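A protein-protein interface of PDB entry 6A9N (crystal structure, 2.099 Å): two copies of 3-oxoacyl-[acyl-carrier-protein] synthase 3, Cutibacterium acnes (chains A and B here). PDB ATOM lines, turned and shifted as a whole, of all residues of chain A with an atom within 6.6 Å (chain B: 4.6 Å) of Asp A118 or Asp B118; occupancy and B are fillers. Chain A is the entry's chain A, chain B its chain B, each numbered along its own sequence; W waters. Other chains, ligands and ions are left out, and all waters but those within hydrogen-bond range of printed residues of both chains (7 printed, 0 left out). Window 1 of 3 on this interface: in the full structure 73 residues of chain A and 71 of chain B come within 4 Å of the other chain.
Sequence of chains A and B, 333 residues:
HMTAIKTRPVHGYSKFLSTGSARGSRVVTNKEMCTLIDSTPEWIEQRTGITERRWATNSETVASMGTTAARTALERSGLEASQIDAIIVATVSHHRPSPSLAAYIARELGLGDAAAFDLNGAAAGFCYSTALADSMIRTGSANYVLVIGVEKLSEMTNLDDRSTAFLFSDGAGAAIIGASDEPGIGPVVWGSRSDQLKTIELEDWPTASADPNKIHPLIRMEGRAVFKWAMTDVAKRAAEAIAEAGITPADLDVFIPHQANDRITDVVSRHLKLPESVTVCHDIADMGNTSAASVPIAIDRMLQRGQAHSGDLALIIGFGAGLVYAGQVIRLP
The backbone carbonyl oxygen (O) of Pro A97 sits at hydrogen-bond distance from the side-chain amide nitrogen (ND2) of Asn B120, 2.9 Å away. The backbone NH (N) of Asn B120 lies within hydrogen-bond range of the backbone carbonyl oxygen (O) of Asp A118, at 2.9 Å. The backbone NH (N) of Asn A120 sits at hydrogen-bond distance from the backbone carbonyl oxygen (O) of Asp B118 (2.9 Å).
The backbone NH of Phe A117 sits at hydrogen-bond distance from the backbone carbonyl oxygen of Ile A87 (3.2 Å). N of Leu A119 sits at hydrogen-bond distance from O of Val A89, at 2.8 Å. The side-chain hydroxyl (OG) of Ser A100 sits at hydrogen-bond distance from the backbone NH (N) of Ala A103 (3.1 Å). OD2 of Asp A118 is in hydrogen-bond range of N of Leu A101 (2.8 Å). The backbone carbonyl oxygen (O) of Val B89 is in hydrogen-bond range of the backbone NH (N) of Leu B119, 2.8 Å away. The backbone carbonyl oxygen of Leu B119 sits at hydrogen-bond distance from the backbone NH of Thr B91 (3.3 Å).
Among the printed residues, merely in contact across the chains: Phe A117 with Asn B120, Leu A119 with Asp B118, Asp A118 with Leu B119, Asn A120 with Phe B117, Phe A117 with Leu B119, Leu A119 with Phe B117, Asn A120 with Ser B100, Ser A100 with Asn B120 and Asp A118 with Asp B118.
Asp A118 touches three residues of chain B. Of chain A, only Asp A118 (3.9 Å), Leu A119 (3.4 Å) and Asn A120 (2.9 Å) come within 4 Å of Asp B118. Of the printed residues of chain B, Leu A119 touches Phe B117 and Asp B118. Printed residues of chain A within 4 Å of Phe B117: Leu A119 and Asn A120. Of the printed residues of chain A, Asn B120 touches Pro A97, Ser A100, Phe A117 and Asp A118. Leu B101 touches none of the printed residues of chain A. The nearest printed residue of chain B that does not touch Asp A118 is Phe B117 (6.2 Å). The nearest residue of chain A that does not touch Asp B118 is Gly A121 (5.4 Å). The nearest printed residue of chain B that does not touch Phe A117 is Phe B117 (5.5 Å).
Printed residues of chain B that touch a printed residue of chain A: Ser B100, Phe B117, Asp B118, Leu B119 and Asn B120. Of the 19 printed residues of chain A, 6 touch a printed residue of chain B. Hydrophobic or aromatic side chains of chain A within 4 Å of the printed part of chain B: Phe A117 and Leu A119. Along chain A the printed residues that touch a printed residue of chain B span positions 97 to 120.
Phe A117 touches Leu B119, and with the chains exchanged Leu A119 touches Phe B117. Phe A117 touches Asn B120, and with the chains exchanged Asn A120 touches Phe B117. Asp A118 touches its own counterpart, Asp B118. Asp A118 touches Leu B119, and with the chains exchanged Leu A119 touches Asp B118. Positions printed for both chains: 89, 91, 94, 100, 101, 102, 117, 118, 119 and 120. Of the 12 pairs that touch across the chains among the printed residues, 11 have their exchanged pair printed and touching as well.
Water W5 lies within hydrogen-bond range of OD1 of Asn A120 (2.6 Å) and N of Ser B100 (3.5 Å). Water W7 bridges OD1 of Asn B120 (2.6 Å) and N of Ser A100 (3.3 Å). Water W3 lies within hydrogen-bond range of the side-chain carboxylate of Asp A118 (2.6 Å) and the side-chain amide nitrogen of Asn B120 (3.2 Å). Water W2 lies within hydrogen-bond range of OG of Ser A100 (2.7 Å), O of Ala A116 (2.8 Å) and O of Asn B120 (2.9 Å). Water W4 bridges the side-chain carboxylate (OD2) of Asp B118 (2.7 Å) and the side-chain amide nitrogen (ND2) of Asn A120 (2.8 Å). Water W6 lies within hydrogen-bond range of the side-chain hydroxyl of Ser B100 (2.8 Å) and the backbone carbonyl oxygen of Asn A120 (2.8 Å).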
ATOM      1  N   ILE A  87     -11.268 -16.757   4.504  1.00  0.00           N
ATOM      2  CA  ILE A  87     -11.468 -17.388   5.802  1.00  0.00           C
ATOM      3  C   ILE A  87     -12.093 -18.756   5.561  1.00  0.00           C
ATOM      4  O   ILE A  87     -13.091 -18.878   4.839  1.00  0.00           O
ATOM      5  CB  ILE A  87     -12.320 -16.521   6.760  1.00  0.00           C
ATOM      6  CG1 ILE A  87     -12.658 -17.303   8.050  1.00  0.00           C
ATOM      7  CG2 ILE A  87     -13.584 -15.970   6.059  1.00  0.00           C
ATOM      8  CD1 ILE A  87     -13.392 -16.479   9.106  1.00  0.00           C
ATOM      9  N   ILE A  88     -11.472 -19.784   6.126  1.00  0.00           N
ATOM     10  CA  ILE A  88     -11.902 -21.168   5.994  1.00  0.00           C
ATOM     11  C   ILE A  88     -12.138 -21.706   7.393  1.00  0.00           C
ATOM     12  O   ILE A  88     -11.241 -21.633   8.244  1.00  0.00           O
ATOM     13  CB  ILE A  88     -10.847 -22.035   5.284  1.00  0.00           C
ATOM     14  CG1 ILE A  88     -10.436 -21.432   3.947  1.00  0.00           C
ATOM     15  CG2 ILE A  88     -11.348 -23.449   5.092  1.00  0.00           C
ATOM     16  CD1 ILE A  88      -9.260 -22.146   3.365  1.00  0.00           C
ATOM     17  N   VAL A  89     -13.314 -22.286   7.618  1.00  0.00           N
ATOM     18  CA  VAL A  89     -13.667 -22.822   8.924  1.00  0.00           C
ATOM     19  C   VAL A  89     -13.925 -24.312   8.770  1.00  0.00           C
ATOM     20  O   VAL A  89     -14.791 -24.715   7.990  1.00  0.00           O
ATOM     21  CB  VAL A  89     -14.882 -22.106   9.532  1.00  0.00           C
ATOM     22  CG1 VAL A  89     -15.235 -22.733  10.873  1.00  0.00           C
ATOM     23  CG2 VAL A  89     -14.583 -20.625   9.711  1.00  0.00           C
ATOM     24  N   ALA A  90     -13.160 -25.119   9.498  1.00  0.00           N
ATOM     25  CA  ALA A  90     -13.311 -26.564   9.509  1.00  0.00           C
ATOM     26  C   ALA A  90     -14.097 -26.945  10.755  1.00  0.00           C
ATOM     27  O   ALA A  90     -13.638 -26.715  11.880  1.00  0.00           O
ATOM     28  CB  ALA A  90     -11.946 -27.254   9.480  1.00  0.00           C
ATOM     29  N   THR A  91     -15.289 -27.500  10.559  1.00  0.00           N
ATOM     30  CA  THR A  91     -16.142 -27.812  11.694  1.00  0.00           C
ATOM     31  C   THR A  91     -17.180 -28.849  11.275  1.00  0.00           C
ATOM     32  O   THR A  91     -17.489 -28.991  10.086  1.00  0.00           O
ATOM     33  CB  THR A  91     -16.819 -26.542  12.241  1.00  0.00           C
ATOM     34  OG1 THR A  91     -17.481 -26.841  13.474  1.00  0.00           O
ATOM     35  CG2 THR A  91     -17.840 -25.966  11.247  1.00  0.00           C
ATOM     36  N   HIS A  94     -21.262 -26.581  13.307  1.00  0.00           N
ATOM     37  CA  HIS A  94     -22.068 -25.426  12.929  1.00  0.00           C
ATOM     38  C   HIS A  94     -23.424 -25.975  12.500  1.00  0.00           C
ATOM     39  O   HIS A  94     -23.582 -26.497  11.386  1.00  0.00           O
ATOM     40  CB  HIS A  94     -21.386 -24.606  11.839  1.00  0.00           C
ATOM     41  CG  HIS A  94     -22.207 -23.450  11.355  1.00  0.00           C
ATOM     42  ND1 HIS A  94     -22.680 -22.464  12.200  1.00  0.00           N
ATOM     43  CD2 HIS A  94     -22.640 -23.125  10.116  1.00  0.00           C
ATOM     44  CE1 HIS A  94     -23.367 -21.580  11.498  1.00  0.00           C
ATOM     45  NE2 HIS A  94     -23.357 -21.961  10.230  1.00  0.00           N
ATOM     46  N   ARG A  96     -26.281 -24.726  11.821  1.00  0.00           N
ATOM     47  CA  ARG A  96     -27.158 -23.958  10.960  1.00  0.00           C
ATOM     48  C   ARG A  96     -26.819 -24.269   9.516  1.00  0.00           C
ATOM     49  O   ARG A  96     -25.635 -24.224   9.163  1.00  0.00           O
ATOM     50  CB  ARG A  96     -26.984 -22.469  11.231  1.00  0.00           C
ATOM     51  CG  ARG A  96     -28.035 -21.605  10.576  1.00  0.00           C
ATOM     52  CD  ARG A  96     -27.690 -20.132  10.722  1.00  0.00           C
ATOM     53  NE  ARG A  96     -27.522 -19.717  12.121  1.00  0.00           N
ATOM     54  CZ  ARG A  96     -28.508 -19.255  12.887  1.00  0.00           C
ATOM     55  NH1 ARG A  96     -29.747 -19.165  12.404  1.00  0.00           N
ATOM     56  NH2 ARG A  96     -28.264 -18.897  14.145  1.00  0.00           N
ATOM     57  N   PRO A  97     -27.783 -24.610   8.651  1.00  0.00           N
ATOM     58  CA  PRO A  97     -27.408 -24.942   7.264  1.00  0.00           C
ATOM     59  C   PRO A  97     -26.699 -23.810   6.543  1.00  0.00           C
ATOM     60  O   PRO A  97     -25.730 -24.050   5.814  1.00  0.00           O
ATOM     61  CB  PRO A  97     -28.756 -25.280   6.604  1.00  0.00           C
ATOM     62  CG  PRO A  97     -29.622 -25.751   7.744  1.00  0.00           C
ATOM     63  CD  PRO A  97     -29.206 -24.880   8.923  1.00  0.00           C
ATOM     64  N   PRO A  99     -26.259 -19.128   6.635  1.00  0.00           N
ATOM     65  CA  PRO A  99     -24.937 -19.106   6.007  1.00  0.00           C
ATOM     66  C   PRO A  99     -23.875 -19.826   6.837  1.00  0.00           C
ATOM     67  O   PRO A  99     -24.149 -20.304   7.944  1.00  0.00           O
ATOM     68  CB  PRO A  99     -24.622 -17.610   5.904  1.00  0.00           C
ATOM     69  CG  PRO A  99     -25.383 -16.985   6.995  1.00  0.00           C
ATOM     70  CD  PRO A  99     -26.643 -17.813   7.167  1.00  0.00           C
ATOM     71  N   SER A 100     -22.663 -19.882   6.293  1.00  0.00           N
ATOM     72  CA  SER A 100     -21.583 -20.652   6.889  1.00  0.00           C
ATOM     73  C   SER A 100     -21.097 -19.992   8.173  1.00  0.00           C
ATOM     74  O   SER A 100     -21.291 -18.797   8.410  1.00  0.00           O
ATOM     75  CB  SER A 100     -20.418 -20.781   5.902  1.00  0.00           C
ATOM     76  OG  SER A 100     -19.912 -19.481   5.593  1.00  0.00           O
ATOM     77  N   LEU A 101     -20.451 -20.795   9.011  1.00  0.00           N
ATOM     78  CA  LEU A 101     -19.780 -20.236  10.180  1.00  0.00           C
ATOM     79  C   LEU A 101     -18.675 -19.271   9.767  1.00  0.00           C
ATOM     80  O   LEU A 101     -18.422 -18.284  10.466  1.00  0.00           O
ATOM     81  CB  LEU A 101     -19.221 -21.360  11.054  1.00  0.00           C
ATOM     82  CG  LEU A 101     -18.652 -20.955  12.426  1.00  0.00           C
ATOM     83  CD1 LEU A 101     -19.631 -20.124  13.228  1.00  0.00           C
ATOM     84  CD2 LEU A 101     -18.255 -22.211  13.198  1.00  0.00           C
ATOM     85  N   ALA A 102     -18.022 -19.521   8.623  1.00  0.00           N
ATOM     86  CA  ALA A 102     -17.045 -18.555   8.115  1.00  0.00           C
ATOM     87  C   ALA A 102     -17.673 -17.182   7.927  1.00  0.00           C
ATOM     88  O   ALA A 102     -17.053 -16.160   8.242  1.00  0.00           O
ATOM     89  CB  ALA A 102     -16.436 -19.041   6.798  1.00  0.00           C
ATOM     90  N   ALA A 103     -18.894 -17.137   7.391  1.00  0.00           N
ATOM     91  CA  ALA A 103     -19.565 -15.855   7.206  1.00  0.00           C
ATOM     92  C   ALA A 103     -19.869 -15.197   8.546  1.00  0.00           C
ATOM     93  O   ALA A 103     -19.701 -13.983   8.689  1.00  0.00           O
ATOM     94  CB  ALA A 103     -20.854 -16.037   6.381  1.00  0.00           C
ATOM     95  N   ALA A 116     -15.063 -16.907   1.683  1.00  0.00           N
ATOM     96  CA  ALA A 116     -15.518 -17.423   2.971  1.00  0.00           C
ATOM     97  C   ALA A 116     -16.288 -18.715   2.752  1.00  0.00           C
ATOM     98  O   ALA A 116     -17.296 -18.733   2.038  1.00  0.00           O
ATOM     99  CB  ALA A 116     -16.382 -16.380   3.709  1.00  0.00           C
ATOM    100  N   PHE A 117     -15.798 -19.802   3.341  1.00  0.00           N
ATOM    101  CA  PHE A 117     -16.522 -21.050   3.244  1.00  0.00           C
ATOM    102  C   PHE A 117     -16.165 -21.932   4.428  1.00  0.00           C
ATOM    103  O   PHE A 117     -15.097 -21.787   5.033  1.00  0.00           O
ATOM    104  CB  PHE A 117     -16.271 -21.765   1.904  1.00  0.00           C
ATOM    105  CG  PHE A 117     -14.827 -22.185   1.664  1.00  0.00           C
ATOM    106  CD1 PHE A 117     -13.942 -21.335   1.015  1.00  0.00           C
ATOM    107  CD2 PHE A 117     -14.385 -23.447   2.032  1.00  0.00           C
ATOM    108  CE1 PHE A 117     -12.632 -21.740   0.737  1.00  0.00           C
ATOM    109  CE2 PHE A 117     -13.069 -23.850   1.772  1.00  0.00           C
ATOM    110  CZ  PHE A 117     -12.202 -22.984   1.123  1.00  0.00           C
ATOM    111  N   ASP A 118     -17.102 -22.813   4.774  1.00  0.00           N
ATOM    112  CA  ASP A 118     -16.891 -23.882   5.742  1.00  0.00           C
ATOM    113  C   ASP A 118     -16.465 -25.137   5.004  1.00  0.00           C
ATOM    114  O   ASP A 118     -16.933 -25.410   3.898  1.00  0.00           O
ATOM    115  CB  ASP A 118     -18.167 -24.231   6.525  1.00  0.00           C
ATOM    116  CG  ASP A 118     -18.625 -23.146   7.480  1.00  0.00           C
ATOM    117  OD1 ASP A 118     -17.851 -22.184   7.741  1.00  0.00           O
ATOM    118  OD2 ASP A 118     -19.783 -23.285   7.994  1.00  0.00           O
ATOM    119  N   LEU A 119     -15.651 -25.952   5.672  1.00  0.00           N
ATOM    120  CA  LEU A 119     -15.223 -27.231   5.142  1.00  0.00           C
ATOM    121  C   LEU A 119     -15.541 -28.330   6.154  1.00  0.00           C
ATOM    122  O   LEU A 119     -15.292 -28.169   7.356  1.00  0.00           O
ATOM    123  CB  LEU A 119     -13.708 -27.187   4.820  1.00  0.00           C
ATOM    124  CG  LEU A 119     -13.013 -28.440   4.296  1.00  0.00           C
ATOM    125  CD1 LEU A 119     -11.865 -28.023   3.404  1.00  0.00           C
ATOM    126  CD2 LEU A 119     -12.502 -29.335   5.428  1.00  0.00           C
ATOM    127  N   ASN A 120     -16.072 -29.457   5.667  1.00  0.00           N
ATOM    128  CA  ASN A 120     -16.350 -30.620   6.508  1.00  0.00           C
ATOM    129  C   ASN A 120     -15.380 -31.726   6.120  1.00  0.00           C
ATOM    130  O   ASN A 120     -15.610 -32.459   5.149  1.00  0.00           O
ATOM    131  CB  ASN A 120     -17.796 -31.105   6.385  1.00  0.00           C
ATOM    132  CG  ASN A 120     -18.101 -32.273   7.346  1.00  0.00           C
ATOM    133  OD1 ASN A 120     -17.198 -32.822   7.996  1.00  0.00           O
ATOM    134  ND2 ASN A 120     -19.373 -32.648   7.442  1.00  0.00           N
ATOM    135  N   GLY A 121     -14.310 -31.845   6.905  1.00  0.00           N
ATOM    136  CA  GLY A 121     -13.329 -32.905   6.779  1.00  0.00           C
ATOM    137  C   GLY A 121     -13.171 -33.699   8.059  1.00  0.00           C
ATOM    138  O   GLY A 121     -12.110 -34.288   8.285  1.00  0.00           O
ATOM    139  N   VAL B  89     -18.134 -31.822  -2.387  1.00  0.00           N
ATOM    140  CA  VAL B  89     -19.587 -31.717  -2.432  1.00  0.00           C
ATOM    141  C   VAL B  89     -19.971 -30.368  -1.860  1.00  0.00           C
ATOM    142  O   VAL B  89     -19.650 -30.063  -0.704  1.00  0.00           O
ATOM    143  CB  VAL B  89     -20.279 -32.855  -1.670  1.00  0.00           C
ATOM    144  CG1 VAL B  89     -21.793 -32.652  -1.688  1.00  0.00           C
ATOM    145  CG2 VAL B  89     -19.910 -34.185  -2.295  1.00  0.00           C
ATOM    146  N   THR B  91     -22.967 -28.062  -0.690  1.00  0.00           N
ATOM    147  CA  THR B  91     -24.332 -28.286  -0.238  1.00  0.00           C
ATOM    148  C   THR B  91     -24.546 -27.521   1.060  1.00  0.00           C
ATOM    149  O   THR B  91     -23.588 -27.206   1.775  1.00  0.00           O
ATOM    150  CB  THR B  91     -24.610 -29.795  -0.058  1.00  0.00           C
ATOM    151  OG1 THR B  91     -26.003 -30.026   0.164  1.00  0.00           O
ATOM    152  CG2 THR B  91     -23.812 -30.376   1.105  1.00  0.00           C
ATOM    153  N   HIS B  94     -26.981 -31.286   3.646  1.00  0.00           N
ATOM    154  CA  HIS B  94     -26.539 -32.528   4.274  1.00  0.00           C
ATOM    155  C   HIS B  94     -26.759 -32.362   5.772  1.00  0.00           C
ATOM    156  O   HIS B  94     -25.967 -31.718   6.459  1.00  0.00           O
ATOM    157  CB  HIS B  94     -25.082 -32.819   3.948  1.00  0.00           C
ATOM    158  CG  HIS B  94     -24.564 -34.075   4.563  1.00  0.00           C
ATOM    159  ND1 HIS B  94     -25.199 -35.291   4.425  1.00  0.00           N
ATOM    160  CD2 HIS B  94     -23.453 -34.309   5.305  1.00  0.00           C
ATOM    161  CE1 HIS B  94     -24.502 -36.221   5.053  1.00  0.00           C
ATOM    162  NE2 HIS B  94     -23.437 -35.652   5.595  1.00  0.00           N
ATOM    163  N   SER B 100     -19.076 -36.583   6.073  1.00  0.00           N
ATOM    164  CA  SER B 100     -19.540 -35.631   5.081  1.00  0.00           C
ATOM    165  C   SER B 100     -20.382 -36.324   4.006  1.00  0.00           C
ATOM    166  O   SER B 100     -20.340 -37.545   3.833  1.00  0.00           O
ATOM    167  CB  SER B 100     -18.343 -34.942   4.423  1.00  0.00           C
ATOM    168  OG  SER B 100     -17.579 -35.903   3.718  1.00  0.00           O
ATOM    169  N   LEU B 101     -21.145 -35.519   3.259  1.00  0.00           N
ATOM    170  CA  LEU B 101     -21.863 -36.073   2.116  1.00  0.00           C
ATOM    171  C   LEU B 101     -20.894 -36.582   1.060  1.00  0.00           C
ATOM    172  O   LEU B 101     -21.175 -37.579   0.384  1.00  0.00           O
ATOM    173  CB  LEU B 101     -22.804 -35.024   1.526  1.00  0.00           C
ATOM    174  CG  LEU B 101     -23.730 -35.511   0.404  1.00  0.00           C
ATOM    175  CD1 LEU B 101     -24.504 -36.765   0.809  1.00  0.00           C
ATOM    176  CD2 LEU B 101     -24.682 -34.408  -0.032  1.00  0.00           C
ATOM    177  N   ALA B 102     -19.739 -35.924   0.918  1.00  0.00           N
ATOM    178  CA  ALA B 102     -18.687 -36.418   0.030  1.00  0.00           C
ATOM    179  C   ALA B 102     -18.309 -37.852   0.371  1.00  0.00           C
ATOM    180  O   ALA B 102     -18.116 -38.686  -0.520  1.00  0.00           O
ATOM    181  CB  ALA B 102     -17.464 -35.492   0.102  1.00  0.00           C
ATOM    182  N   PHE B 117     -14.304 -33.903   0.934  1.00  0.00           N
ATOM    183  CA  PHE B 117     -14.827 -32.932   1.884  1.00  0.00           C
ATOM    184  C   PHE B 117     -16.069 -32.266   1.315  1.00  0.00           C
ATOM    185  O   PHE B 117     -16.252 -32.208   0.098  1.00  0.00           O
ATOM    186  CB  PHE B 117     -13.770 -31.877   2.289  1.00  0.00           C
ATOM    187  CG  PHE B 117     -13.227 -31.032   1.141  1.00  0.00           C
ATOM    188  CD1 PHE B 117     -12.119 -31.448   0.409  1.00  0.00           C
ATOM    189  CD2 PHE B 117     -13.779 -29.787   0.855  1.00  0.00           C
ATOM    190  CE1 PHE B 117     -11.604 -30.653  -0.625  1.00  0.00           C
ATOM    191  CE2 PHE B 117     -13.268 -28.979  -0.164  1.00  0.00           C
ATOM    192  CZ  PHE B 117     -12.178 -29.413  -0.900  1.00  0.00           C
ATOM    193  N   ASP B 118     -16.954 -31.829   2.224  1.00  0.00           N
ATOM    194  CA  ASP B 118     -18.083 -30.955   1.923  1.00  0.00           C
ATOM    195  C   ASP B 118     -17.645 -29.503   2.058  1.00  0.00           C
ATOM    196  O   ASP B 118     -16.864 -29.155   2.941  1.00  0.00           O
ATOM    197  CB  ASP B 118     -19.261 -31.167   2.888  1.00  0.00           C
ATOM    198  CG  ASP B 118     -19.984 -32.503   2.703  1.00  0.00           C
ATOM    199  OD1 ASP B 118     -19.636 -33.256   1.758  1.00  0.00           O
ATOM    200  OD2 ASP B 118     -20.921 -32.790   3.522  1.00  0.00           O
ATOM    201  N   LEU B 119     -18.218 -28.645   1.226  1.00  0.00           N
ATOM    202  CA  LEU B 119     -17.953 -27.217   1.246  1.00  0.00           C
ATOM    203  C   LEU B 119     -19.278 -26.486   1.393  1.00  0.00           C
ATOM    204  O   LEU B 119     -20.240 -26.805   0.686  1.00  0.00           O
ATOM    205  CB  LEU B 119     -17.236 -26.783  -0.048  1.00  0.00           C
ATOM    206  CG  LEU B 119     -16.872 -25.308  -0.166  1.00  0.00           C
ATOM    207  CD1 LEU B 119     -15.540 -25.204  -0.871  1.00  0.00           C
ATOM    208  CD2 LEU B 119     -17.942 -24.493  -0.902  1.00  0.00           C
ATOM    209  N   ASN B 120     -19.330 -25.498   2.297  1.00  0.00           N
ATOM    210  CA  ASN B 120     -20.506 -24.644   2.446  1.00  0.00           C
ATOM    211  C   ASN B 120     -20.131 -23.262   1.928  1.00  0.00           C
ATOM    212  O   ASN B 120     -19.465 -22.484   2.624  1.00  0.00           O
ATOM    213  CB  ASN B 120     -20.999 -24.576   3.892  1.00  0.00           C
ATOM    214  CG  ASN B 120     -22.291 -23.766   4.026  1.00  0.00           C
ATOM    215  OD1 ASN B 120     -22.746 -23.134   3.067  1.00  0.00           O
ATOM    216  ND2 ASN B 120     -22.883 -23.779   5.219  1.00  0.00           N
HETATM  217  O   HOH W   1     -24.617 -26.525   5.906  1.00  0.00           O
HETATM  218  O   HOH W   2     -19.764 -19.586   2.948  1.00  0.00           O
HETATM  219  O   HOH W   3     -21.300 -25.340   7.467  1.00  0.00           O
HETATM  220  O   HOH W   4     -21.234 -31.453   5.804  1.00  0.00           O
HETATM  221  O   HOH W   5     -17.261 -35.298   8.748  1.00  0.00           O
HETATM  222  O   HOH W   6     -15.044 -35.155   4.565  1.00  0.00           O
HETATM  223  O   HOH W   7     -24.155 -21.008   3.529  1.00  0.00           O
